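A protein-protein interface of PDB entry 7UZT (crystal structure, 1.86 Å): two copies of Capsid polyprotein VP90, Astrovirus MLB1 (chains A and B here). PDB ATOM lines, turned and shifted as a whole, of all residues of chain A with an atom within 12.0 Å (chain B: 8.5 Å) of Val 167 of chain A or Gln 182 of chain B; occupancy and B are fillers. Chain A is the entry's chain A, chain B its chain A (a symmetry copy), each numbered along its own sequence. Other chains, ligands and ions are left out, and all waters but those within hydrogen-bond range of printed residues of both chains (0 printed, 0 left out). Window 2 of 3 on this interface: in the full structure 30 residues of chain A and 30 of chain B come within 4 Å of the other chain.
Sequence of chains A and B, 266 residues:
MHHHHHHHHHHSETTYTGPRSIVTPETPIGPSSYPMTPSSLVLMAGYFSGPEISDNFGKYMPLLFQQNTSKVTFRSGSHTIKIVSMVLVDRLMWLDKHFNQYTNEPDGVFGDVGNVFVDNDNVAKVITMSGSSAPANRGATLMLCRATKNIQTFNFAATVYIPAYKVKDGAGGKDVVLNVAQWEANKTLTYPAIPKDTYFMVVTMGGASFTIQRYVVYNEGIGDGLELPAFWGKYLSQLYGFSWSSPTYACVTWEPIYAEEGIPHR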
ATOM      1  N   ILE A 162      28.216 -17.100  27.341  1.00  0.00           N
ATOM      2  CA  ILE A 162      27.365 -17.549  28.430  1.00  0.00           C
ATOM      3  C   ILE A 162      26.065 -18.036  27.810  1.00  0.00           C
ATOM      4  O   ILE A 162      25.349 -17.248  27.186  1.00  0.00           O
ATOM      5  CB  ILE A 162      27.109 -16.428  29.453  1.00  0.00           C
ATOM      6  CG1 ILE A 162      28.379 -16.209  30.275  1.00  0.00           C
ATOM      7  CG2 ILE A 162      25.922 -16.757  30.352  1.00  0.00           C
ATOM      8  CD1 ILE A 162      28.558 -14.825  30.733  1.00  0.00           C
ATOM      9  N   PRO A 163      25.720 -19.315  27.933  1.00  0.00           N
ATOM     10  CA  PRO A 163      24.466 -19.802  27.351  1.00  0.00           C
ATOM     11  C   PRO A 163      23.328 -19.538  28.323  1.00  0.00           C
ATOM     12  O   PRO A 163      23.414 -19.890  29.501  1.00  0.00           O
ATOM     13  CB  PRO A 163      24.716 -21.304  27.177  1.00  0.00           C
ATOM     14  CG  PRO A 163      25.650 -21.631  28.267  1.00  0.00           C
ATOM     15  CD  PRO A 163      26.547 -20.416  28.452  1.00  0.00           C
ATOM     16  N   ALA A 164      22.249 -18.945  27.831  1.00  0.00           N
ATOM     17  CA  ALA A 164      21.194 -18.566  28.760  1.00  0.00           C
ATOM     18  C   ALA A 164      19.898 -18.408  27.995  1.00  0.00           C
ATOM     19  O   ALA A 164      19.903 -17.995  26.834  1.00  0.00           O
ATOM     20  CB  ALA A 164      21.546 -17.270  29.508  1.00  0.00           C
ATOM     21  N   TYR A 165      18.793 -18.767  28.635  1.00  0.00           N
ATOM     22  CA  TYR A 165      17.501 -18.565  28.001  1.00  0.00           C
ATOM     23  C   TYR A 165      17.263 -17.078  27.821  1.00  0.00           C
ATOM     24  O   TYR A 165      17.591 -16.269  28.695  1.00  0.00           O
ATOM     25  CB  TYR A 165      16.372 -19.126  28.834  1.00  0.00           C
ATOM     26  CG  TYR A 165      16.265 -20.617  28.842  1.00  0.00           C
ATOM     27  CD1 TYR A 165      16.260 -21.336  27.669  1.00  0.00           C
ATOM     28  CD2 TYR A 165      16.024 -21.288  30.016  1.00  0.00           C
ATOM     29  CE1 TYR A 165      16.111 -22.717  27.664  1.00  0.00           C
ATOM     30  CE2 TYR A 165      15.871 -22.651  30.034  1.00  0.00           C
ATOM     31  CZ  TYR A 165      15.915 -23.372  28.859  1.00  0.00           C
ATOM     32  OH  TYR A 165      15.759 -24.746  28.897  1.00  0.00           O
ATOM     33  N   LYS A 166      16.649 -16.735  26.698  1.00  0.00           N
ATOM     34  CA  LYS A 166      16.441 -15.356  26.293  1.00  0.00           C
ATOM     35  C   LYS A 166      15.044 -15.255  25.718  1.00  0.00           C
ATOM     36  O   LYS A 166      14.624 -16.123  24.944  1.00  0.00           O
ATOM     37  CB  LYS A 166      17.488 -14.905  25.267  1.00  0.00           C
ATOM     38  CG  LYS A 166      17.050 -13.758  24.375  1.00  0.00           C
ATOM     39  CD  LYS A 166      18.238 -12.916  23.942  1.00  0.00           C
ATOM     40  CE  LYS A 166      17.813 -11.469  23.676  1.00  0.00           C
ATOM     41  NZ  LYS A 166      17.797 -11.144  22.214  1.00  0.00           N
ATOM     42  N   VAL A 167      14.404 -14.222  26.132  1.00  0.00           N
ATOM     43  CA  VAL A 167      13.018 -14.098  25.722  1.00  0.00           C
ATOM     44  C   VAL A 167      12.956 -13.435  24.350  1.00  0.00           C
ATOM     45  O   VAL A 167      13.696 -12.484  24.077  1.00  0.00           O
ATOM     46  CB  VAL A 167      12.197 -13.311  26.761  1.00  0.00           C
ATOM     47  CG1 VAL A 167      10.775 -13.085  26.256  1.00  0.00           C
ATOM     48  CG2 VAL A 167      12.189 -14.039  28.089  1.00  0.00           C
ATOM     49  N   VAL A 176      10.872 -18.480  23.654  1.00  0.00           N
ATOM     50  CA  VAL A 176      12.102 -18.423  24.443  1.00  0.00           C
ATOM     51  C   VAL A 176      13.145 -19.243  23.711  1.00  0.00           C
ATOM     52  O   VAL A 176      12.818 -20.281  23.143  1.00  0.00           O
ATOM     53  CB  VAL A 176      11.897 -18.987  25.860  1.00  0.00           C
ATOM     54  CG1 VAL A 176      13.250 -19.120  26.584  1.00  0.00           C
ATOM     55  CG2 VAL A 176      10.931 -18.120  26.613  1.00  0.00           C
ATOM     56  N   VAL A 177      14.320 -18.818  23.720  1.00  0.00           N
ATOM     57  CA  VAL A 177      15.428 -19.531  23.052  1.00  0.00           C
ATOM     58  C   VAL A 177      16.637 -19.639  23.981  1.00  0.00           C
ATOM     59  O   VAL A 177      16.780 -18.807  24.878  1.00  0.00           O
ATOM     60  CB  VAL A 177      15.796 -18.794  21.758  1.00  0.00           C
ATOM     61  CG1 VAL A 177      14.652 -18.803  20.754  1.00  0.00           C
ATOM     62  CG2 VAL A 177      16.269 -17.376  22.017  1.00  0.00           C
ATOM     63  N   LEU A 178      17.524 -20.561  23.569  1.00  0.00           N
ATOM     64  CA  LEU A 178      18.800 -20.720  24.256  1.00  0.00           C
ATOM     65  C   LEU A 178      19.803 -19.835  23.536  1.00  0.00           C
ATOM     66  O   LEU A 178      20.310 -20.184  22.460  1.00  0.00           O
ATOM     67  CB  LEU A 178      19.258 -22.175  24.252  1.00  0.00           C
ATOM     68  CG  LEU A 178      20.152 -22.646  25.393  1.00  0.00           C
ATOM     69  CD1 LEU A 178      20.101 -24.192  25.480  1.00  0.00           C
ATOM     70  CD2 LEU A 178      21.593 -22.100  25.245  1.00  0.00           C
ATOM     71  N   ASN A 179      20.116 -18.704  24.145  1.00  0.00           N
ATOM     72  CA  ASN A 179      20.973 -17.694  23.554  1.00  0.00           C
ATOM     73  C   ASN A 179      22.411 -17.932  23.992  1.00  0.00           C
ATOM     74  O   ASN A 179      22.688 -18.120  25.177  1.00  0.00           O
ATOM     75  CB  ASN A 179      20.487 -16.306  23.968  1.00  0.00           C
ATOM     76  CG  ASN A 179      21.238 -15.185  23.289  1.00  0.00           C
ATOM     77  OD1 ASN A 179      22.188 -14.627  23.851  1.00  0.00           O
ATOM     78  ND2 ASN A 179      20.820 -14.837  22.073  1.00  0.00           N
ATOM     79  N   VAL A 180      23.326 -17.963  23.032  1.00  0.00           N
ATOM     80  CA  VAL A 180      24.744 -18.060  23.338  1.00  0.00           C
ATOM     81  C   VAL A 180      25.248 -16.630  23.212  1.00  0.00           C
ATOM     82  O   VAL A 180      25.537 -16.142  22.114  1.00  0.00           O
ATOM     83  CB  VAL A 180      25.471 -19.048  22.417  1.00  0.00           C
ATOM     84  CG1 VAL A 180      26.877 -19.210  22.838  1.00  0.00           C
ATOM     85  CG2 VAL A 180      24.767 -20.405  22.482  1.00  0.00           C
ATOM     86  N   ALA A 181      25.277 -15.933  24.341  1.00  0.00           N
ATOM     87  CA  ALA A 181      25.601 -14.520  24.369  1.00  0.00           C
ATOM     88  C   ALA A 181      27.099 -14.339  24.547  1.00  0.00           C
ATOM     89  O   ALA A 181      27.696 -14.893  25.475  1.00  0.00           O
ATOM     90  CB  ALA A 181      24.838 -13.809  25.493  1.00  0.00           C
ATOM     91  N   LEU A 226      24.702 -16.970  18.657  1.00  0.00           N
ATOM     92  CA  LEU A 226      23.897 -18.144  18.227  1.00  0.00           C
ATOM     93  C   LEU A 226      22.685 -18.350  19.130  1.00  0.00           C
ATOM     94  O   LEU A 226      22.813 -18.197  20.340  1.00  0.00           O
ATOM     95  CB  LEU A 226      24.772 -19.394  18.284  1.00  0.00           C
ATOM     96  CG  LEU A 226      24.207 -20.657  17.640  1.00  0.00           C
ATOM     97  CD1 LEU A 226      23.941 -20.438  16.163  1.00  0.00           C
ATOM     98  CD2 LEU A 226      25.170 -21.814  17.834  1.00  0.00           C
ATOM     99  N   GLU A 227      21.565 -18.711  18.535  1.00  0.00           N
ATOM    100  CA  GLU A 227      20.361 -19.020  19.312  1.00  0.00           C
ATOM    101  C   GLU A 227      19.971 -20.458  19.000  1.00  0.00           C
ATOM    102  O   GLU A 227      19.800 -20.787  17.821  1.00  0.00           O
ATOM    103  CB  GLU A 227      19.252 -18.035  18.963  1.00  0.00           C
ATOM    104  CG  GLU A 227      17.875 -18.643  19.044  1.00  0.00           C
ATOM    105  CD  GLU A 227      16.935 -18.455  17.873  1.00  0.00           C
ATOM    106  OE1 GLU A 227      16.566 -17.300  17.602  1.00  0.00           O
ATOM    107  OE2 GLU A 227      16.547 -19.470  17.267  1.00  0.00           O
ATOM    108  N   LEU A 228      19.926 -21.286  20.019  1.00  0.00           N
ATOM    109  CA  LEU A 228      19.493 -22.683  19.874  1.00  0.00           C
ATOM    110  C   LEU A 228      18.059 -22.777  20.391  1.00  0.00           C
ATOM    111  O   LEU A 228      17.688 -22.015  21.272  1.00  0.00           O
ATOM    112  CB  LEU A 228      20.397 -23.586  20.714  1.00  0.00           C
ATOM    113  CG  LEU A 228      21.882 -23.648  20.395  1.00  0.00           C
ATOM    114  CD1 LEU A 228      22.549 -24.660  21.309  1.00  0.00           C
ATOM    115  CD2 LEU A 228      22.111 -24.021  18.947  1.00  0.00           C
ATOM    116  N   PRO A 229      17.239 -23.693  19.872  1.00  0.00           N
ATOM    117  CA  PRO A 229      15.879 -23.887  20.366  1.00  0.00           C
ATOM    118  C   PRO A 229      15.942 -24.231  21.842  1.00  0.00           C
ATOM    119  O   PRO A 229      16.896 -24.863  22.309  1.00  0.00           O
ATOM    120  CB  PRO A 229      15.361 -25.058  19.526  1.00  0.00           C
ATOM    121  CG  PRO A 229      16.164 -24.957  18.237  1.00  0.00           C
ATOM    122  CD  PRO A 229      17.539 -24.563  18.719  1.00  0.00           C
ATOM    123  N   ALA A 230      14.928 -23.801  22.584  1.00  0.00           N
ATOM    124  CA  ALA A 230      14.905 -24.023  24.051  1.00  0.00           C
ATOM    125  C   ALA A 230      14.950 -25.522  24.360  1.00  0.00           C
ATOM    126  O   ALA A 230      15.366 -25.851  25.479  1.00  0.00           O
ATOM    127  CB  ALA A 230      13.678 -23.392  24.632  1.00  0.00           C
ATOM    128  N   MET B  61      10.111 -25.829  32.396  1.00  0.00           N
ATOM    129  CA  MET B  61      10.820 -24.534  32.342  1.00  0.00           C
ATOM    130  C   MET B  61      10.957 -23.945  33.743  1.00  0.00           C
ATOM    131  O   MET B  61       9.929 -23.564  34.320  1.00  0.00           O
ATOM    132  CB  MET B  61      10.031 -23.528  31.496  1.00  0.00           C
ATOM    133  CG  MET B  61      10.919 -22.610  30.689  1.00  0.00           C
ATOM    134  SD  MET B  61      11.746 -23.472  29.331  1.00  0.00           S
ATOM    135  CE  MET B  61      11.898 -22.130  28.154  1.00  0.00           C
ATOM    136  N   LEU B  64       9.996 -17.930  37.307  1.00  0.00           N
ATOM    137  CA  LEU B  64       9.531 -17.125  38.422  1.00  0.00           C
ATOM    138  C   LEU B  64       8.199 -16.485  38.040  1.00  0.00           C
ATOM    139  O   LEU B  64       7.883 -16.306  36.854  1.00  0.00           O
ATOM    140  CB  LEU B  64      10.540 -16.022  38.771  1.00  0.00           C
ATOM    141  CG  LEU B  64      11.960 -16.460  39.128  1.00  0.00           C
ATOM    142  CD1 LEU B  64      12.889 -15.235  39.231  1.00  0.00           C
ATOM    143  CD2 LEU B  64      11.991 -17.353  40.378  1.00  0.00           C
ATOM    144  N   GLN B  66       5.182 -13.229  39.222  1.00  0.00           N
ATOM    145  CA  GLN B  66       4.799 -12.079  40.055  1.00  0.00           C
ATOM    146  C   GLN B  66       3.282 -12.150  40.098  1.00  0.00           C
ATOM    147  O   GLN B  66       2.673 -11.895  39.067  1.00  0.00           O
ATOM    148  CB  GLN B  66       5.290 -10.782  39.429  1.00  0.00           C
ATOM    149  CG  GLN B  66       4.651  -9.531  40.003  1.00  0.00           C
ATOM    150  CD  GLN B  66       5.740  -8.602  40.464  1.00  0.00           C
ATOM    151  OE1 GLN B  66       6.500  -8.931  41.366  1.00  0.00           O
ATOM    152  NE2 GLN B  66       5.845  -7.456  39.815  1.00  0.00           N
ATOM    153  N   ALA B 158      -0.704 -14.229  37.131  1.00  0.00           N
ATOM    154  CA  ALA B 158       0.647 -13.792  37.433  1.00  0.00           C
ATOM    155  C   ALA B 158       1.338 -13.478  36.130  1.00  0.00           C
ATOM    156  O   ALA B 158       0.986 -14.029  35.091  1.00  0.00           O
ATOM    157  CB  ALA B 158       1.428 -14.868  38.201  1.00  0.00           C
ATOM    158  N   THR B 159       2.295 -12.564  36.189  1.00  0.00           N
ATOM    159  CA  THR B 159       3.251 -12.420  35.112  1.00  0.00           C
ATOM    160  C   THR B 159       4.286 -13.520  35.305  1.00  0.00           C
ATOM    161  O   THR B 159       4.620 -13.880  36.440  1.00  0.00           O
ATOM    162  CB  THR B 159       3.895 -11.027  35.135  1.00  0.00           C
ATOM    163  OG1 THR B 159       2.885 -10.029  34.901  1.00  0.00           O
ATOM    164  CG2 THR B 159       4.938 -10.891  34.062  1.00  0.00           C
ATOM    165  N   VAL B 160       4.721 -14.124  34.213  1.00  0.00           N
ATOM    166  CA  VAL B 160       5.657 -15.238  34.288  1.00  0.00           C
ATOM    167  C   VAL B 160       6.999 -14.745  33.790  1.00  0.00           C
ATOM    168  O   VAL B 160       7.081 -14.013  32.794  1.00  0.00           O
ATOM    169  CB  VAL B 160       5.158 -16.472  33.511  1.00  0.00           C
ATOM    170  CG1 VAL B 160       6.294 -17.468  33.289  1.00  0.00           C
ATOM    171  CG2 VAL B 160       4.093 -17.157  34.326  1.00  0.00           C
ATOM    172  N   TYR B 161       8.039 -15.116  34.519  1.00  0.00           N
ATOM    173  CA  TYR B 161       9.400 -14.661  34.295  1.00  0.00           C
ATOM    174  C   TYR B 161      10.356 -15.837  34.184  1.00  0.00           C
ATOM    175  O   TYR B 161      10.168 -16.882  34.801  1.00  0.00           O
ATOM    176  CB  TYR B 161       9.886 -13.798  35.427  1.00  0.00           C
ATOM    177  CG  TYR B 161       9.120 -12.536  35.625  1.00  0.00           C
ATOM    178  CD1 TYR B 161       9.482 -11.386  34.957  1.00  0.00           C
ATOM    179  CD2 TYR B 161       8.029 -12.494  36.473  1.00  0.00           C
ATOM    180  CE1 TYR B 161       8.786 -10.202  35.145  1.00  0.00           C
ATOM    181  CE2 TYR B 161       7.328 -11.326  36.673  1.00  0.00           C
ATOM    182  CZ  TYR B 161       7.706 -10.180  35.997  1.00  0.00           C
ATOM    183  OH  TYR B 161       7.000  -9.011  36.193  1.00  0.00           O
ATOM    184  N   ILE B 162      11.422 -15.614  33.435  1.00  0.00           N
ATOM    185  CA  ILE B 162      12.475 -16.599  33.251  1.00  0.00           C
ATOM    186  C   ILE B 162      13.758 -15.988  33.793  1.00  0.00           C
ATOM    187  O   ILE B 162      14.219 -14.967  33.275  1.00  0.00           O
ATOM    188  CB  ILE B 162      12.629 -17.000  31.773  1.00  0.00           C
ATOM    189  CG1 ILE B 162      11.455 -17.893  31.378  1.00  0.00           C
ATOM    190  CG2 ILE B 162      13.961 -17.699  31.525  1.00  0.00           C
ATOM    191  CD1 ILE B 162      11.064 -17.770  29.967  1.00  0.00           C
ATOM    192  N   PRO B 163      14.362 -16.554  34.835  1.00  0.00           N
ATOM    193  CA  PRO B 163      15.605 -15.986  35.366  1.00  0.00           C
ATOM    194  C   PRO B 163      16.780 -16.517  34.564  1.00  0.00           C
ATOM    195  O   PRO B 163      16.914 -17.728  34.372  1.00  0.00           O
ATOM    196  CB  PRO B 163      15.638 -16.496  36.812  1.00  0.00           C
ATOM    197  CG  PRO B 163      14.931 -17.786  36.743  1.00  0.00           C
ATOM    198  CD  PRO B 163      13.842 -17.631  35.692  1.00  0.00           C
ATOM    199  N   ALA B 164      17.650 -15.623  34.115  1.00  0.00           N
ATOM    200  CA  ALA B 164      18.717 -16.085  33.239  1.00  0.00           C
ATOM    201  C   ALA B 164      19.849 -15.082  33.271  1.00  0.00           C
ATOM    202  O   ALA B 164      19.617 -13.881  33.412  1.00  0.00           O
ATOM    203  CB  ALA B 164      18.212 -16.290  31.802  1.00  0.00           C
ATOM    204  N   ASN B 179      19.214 -11.819  35.247  1.00  0.00           N
ATOM    205  CA  ASN B 179      18.106 -11.049  34.714  1.00  0.00           C
ATOM    206  C   ASN B 179      16.811 -11.822  34.914  1.00  0.00           C
ATOM    207  O   ASN B 179      16.727 -13.009  34.598  1.00  0.00           O
ATOM    208  CB  ASN B 179      18.355 -10.753  33.235  1.00  0.00           C
ATOM    209  CG  ASN B 179      17.318  -9.837  32.628  1.00  0.00           C
ATOM    210  OD1 ASN B 179      16.355 -10.297  32.005  1.00  0.00           O
ATOM    211  ND2 ASN B 179      17.503  -8.529  32.799  1.00  0.00           N
ATOM    212  N   VAL B 180      15.807 -11.161  35.476  1.00  0.00           N
ATOM    213  CA  VAL B 180      14.486 -11.754  35.606  1.00  0.00           C
ATOM    214  C   VAL B 180      13.697 -11.156  34.451  1.00  0.00           C
ATOM    215  O   VAL B 180      13.182 -10.035  34.533  1.00  0.00           O
ATOM    216  CB  VAL B 180      13.860 -11.483  36.980  1.00  0.00           C
ATOM    217  CG1 VAL B 180      12.579 -12.203  37.115  1.00  0.00           C
ATOM    218  CG2 VAL B 180      14.822 -11.957  38.071  1.00  0.00           C
ATOM    219  N   ALA B 181      13.672 -11.882  33.340  1.00  0.00           N
ATOM    220  CA  ALA B 181      13.081 -11.392  32.110  1.00  0.00           C
ATOM    221  C   ALA B 181      11.611 -11.773  32.058  1.00  0.00           C
ATOM    222  O   ALA B 181      11.256 -12.945  32.221  1.00  0.00           O
ATOM    223  CB  ALA B 181      13.822 -11.950  30.889  1.00  0.00           C
ATOM    224  N   GLN B 182      10.757 -10.783  31.811  1.00  0.00           N
ATOM    225  CA  GLN B 182       9.348 -11.076  31.645  1.00  0.00           C
ATOM    226  C   GLN B 182       9.114 -11.870  30.368  1.00  0.00           C
ATOM    227  O   GLN B 182       9.687 -11.571  29.315  1.00  0.00           O
ATOM    228  CB  GLN B 182       8.541  -9.780  31.642  1.00  0.00           C
ATOM    229  CG  GLN B 182       7.162  -9.952  31.103  1.00  0.00           C
ATOM    230  CD  GLN B 182       6.430  -8.641  31.029  1.00  0.00           C
ATOM    231  OE1 GLN B 182       6.574  -7.793  31.908  1.00  0.00           O
ATOM    232  NE2 GLN B 182       5.688  -8.438  29.948  1.00  0.00           N
ATOM    233  N   TRP B 183       8.251 -12.875  30.468  1.00  0.00           N
ATOM    234  CA  TRP B 183       7.868 -13.736  29.362  1.00  0.00           C
ATOM    235  C   TRP B 183       6.482 -13.340  28.883  1.00  0.00           C
ATOM    236  O   TRP B 183       6.334 -12.771  27.797  1.00  0.00           O
ATOM    237  CB  TRP B 183       7.892 -15.209  29.787  1.00  0.00           C
ATOM    238  CG  TRP B 183       7.817 -16.183  28.629  1.00  0.00           C
ATOM    239  CD1 TRP B 183       7.881 -15.880  27.292  1.00  0.00           C
ATOM    240  CD2 TRP B 183       7.675 -17.608  28.710  1.00  0.00           C
ATOM    241  NE1 TRP B 183       7.785 -17.026  26.544  1.00  0.00           N
ATOM    242  CE2 TRP B 183       7.654 -18.101  27.387  1.00  0.00           C
ATOM    243  CE3 TRP B 183       7.560 -18.516  29.768  1.00  0.00           C
ATOM    244  CZ2 TRP B 183       7.529 -19.465  27.098  1.00  0.00           C
ATOM    245  CZ3 TRP B 183       7.426 -19.863  29.479  1.00  0.00           C
ATOM    246  CH2 TRP B 183       7.415 -20.325  28.154  1.00  0.00           C
ATOM    247  N   GLU B 184       5.461 -13.613  29.689  1.00  0.00           N
ATOM    248  CA  GLU B 184       4.110 -13.232  29.316  1.00  0.00           C
ATOM    249  C   GLU B 184       3.332 -12.764  30.536  1.00  0.00           C
ATOM    250  O   GLU B 184       3.360 -13.398  31.596  1.00  0.00           O
ATOM    251  CB  GLU B 184       3.377 -14.388  28.619  1.00  0.00           C
ATOM    252  CG  GLU B 184       3.363 -14.240  27.093  1.00  0.00           C
ATOM    253  CD  GLU B 184       2.243 -13.334  26.597  1.00  0.00           C
ATOM    254  OE1 GLU B 184       1.051 -13.703  26.754  1.00  0.00           O
ATOM    255  OE2 GLU B 184       2.559 -12.239  26.075  1.00  0.00           O
ATOM    256  N   ALA B 185       2.639 -11.644  30.371  1.00  0.00           N
ATOM    257  CA  ALA B 185       1.803 -11.108  31.423  1.00  0.00           C
ATOM    258  C   ALA B 185       0.465 -11.837  31.463  1.00  0.00           C
ATOM    259  O   ALA B 185       0.021 -12.429  30.477  1.00  0.00           O
ATOM    260  CB  ALA B 185       1.590  -9.605  31.229  1.00  0.00           C
ATOM    261  N   ASN B 186      -0.183 -11.771  32.618  1.00  0.00           N
ATOM    262  CA  ASN B 186      -1.557 -12.303  32.804  1.00  0.00           C
ATOM    263  C   ASN B 186      -1.756 -13.742  32.330  1.00  0.00           C
ATOM    264  O   ASN B 186      -2.563 -13.960  31.438  1.00  0.00           O
ATOM    265  CB  ASN B 186      -2.619 -11.336  32.259  1.00  0.00           C
ATOM    266  CG  ASN B 186      -3.377 -10.680  33.392  1.00  0.00           C
ATOM    267  OD1 ASN B 186      -4.061 -11.356  34.156  1.00  0.00           O
ATOM    268  ND2 ASN B 186      -3.225  -9.375  33.532  1.00  0.00           N
ATOM    269  N   LEU B 226      13.725  -7.131  36.678  1.00  0.00           N
ATOM    270  CA  LEU B 226      14.686  -7.069  37.811  1.00  0.00           C
ATOM    271  C   LEU B 226      16.018  -7.718  37.447  1.00  0.00           C
ATOM    272  O   LEU B 226      16.015  -8.758  36.798  1.00  0.00           O
ATOM    273  CB  LEU B 226      14.091  -7.806  39.009  1.00  0.00           C
ATOM    274  CG  LEU B 226      14.809  -7.638  40.344  1.00  0.00           C
ATOM    275  CD1 LEU B 226      14.839  -6.180  40.762  1.00  0.00           C
ATOM    276  CD2 LEU B 226      14.127  -8.475  41.411  1.00  0.00           C
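The backbone carbonyl oxygen (O) of Val 160 of chain B lies within hydrogen-bond range of the backbone NH (N) of Trp 183 of chain B.
The backbone NH (N) of Ile 162 of chain B is in hydrogen-bond range of the backbone carbonyl oxygen (O) of Ala 181 of chain B (2.9 Å).
O of Ala 164 of chain B sits at hydrogen-bond distance from N of Asn 179 of chain B (2.8 Å).
N of Ala 181 of chain B lies close to OD1 of Asn 179 of chain B (3.4 Å).
Of the printed residues of chain B, Tyr 165 of chain A touches Ile 162 (3.9 Å) and Ala 164 (3.2 Å).
Val 167 of chain A touches just these residues of chain B: Ala 181 and Gln 182.
Leu 228 of chain A touches none of the printed residues of chain B.
No residue of chain A comes within 4 Å of Thr 159 of chain B.
No residue of chain A comes within 4 Å of Tyr 161 of chain B.
Of chain A, only Tyr 165 and Val 176 come within 4 Å of Ile 162 of chain B.
Printed residues of chain A within 4 Å of Ala 164 of chain B: Tyr 165.
Val 180 of chain B touches none of the printed residues of chain A.
Ala 181 of chain B touches one residue of chain A.
Gln 182 of chain B touches just one residue of chain A: Val 167.
Of chain A, only Val 176 (3.3 Å) comes within 4 Å of Trp 183 of chain B.
Glu 184 of chain B touches none of the printed residues of chain A.
The nearest residue of chain B that does not touch Val 167 of chain A is Trp 183 of chain B (4.2 Å).
The nearest residue of chain A that does not touch Gln 182 of chain B is Val 176 of chain A (7.2 Å).
Ile 162 of chain B touches Tyr 165 of chain A (CG2 to CB, 3.9 Å).
Ala 164 of chain B touches Tyr 165 of chain A.
Val 167 of chain A touches Ala 181 of chain B.
Gln 182 of chain B touches Val 167 of chain A.
Val 176 of chain A touches Met 61 of chain B (CG1 to CE, 3.7 Å).
CD1 of Ile 162 of chain B touches CG2 of Val 176 of chain A, at 3.4 Å.
NE1 of Trp 183 of chain B touches CG2 of Val 176 of chain A, at 3.3 Å.
Positions printed for both chains: 162, 163, 164, 179, 180, 181 and 226.
Of the 7 pairs that touch across the chains among the printed residues, none has its exchanged pair printed and touching as well.
Of the 17 printed residues of chain A, 3 touch a printed residue of chain B.
Printed residues of chain A that touch a printed residue of chain B: Tyr 165, Val 167 and Val 176.
Hydrophobic or aromatic side chains of chain A within 4 Å of the printed part of chain B: Tyr 165, Val 167 and Val 176.
Of the 19 printed residues of chain B, 6 touch a printed residue of chain A.
Printed residues of chain B that touch a printed residue of chain A: Met 61, Ile 162, Ala 164, Ala 181, Gln 182 and Trp 183.
Hydrophobic or aromatic side chains of chain B within 4 Å of the printed part of chain A: Met 61, Ile 162, Ala 164, Ala 181 and Trp 183.
Among the printed residues, no Asp or Glu carboxylate lies within 4 Å of a Lys or Arg side-chain nitrogen of the other chain.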
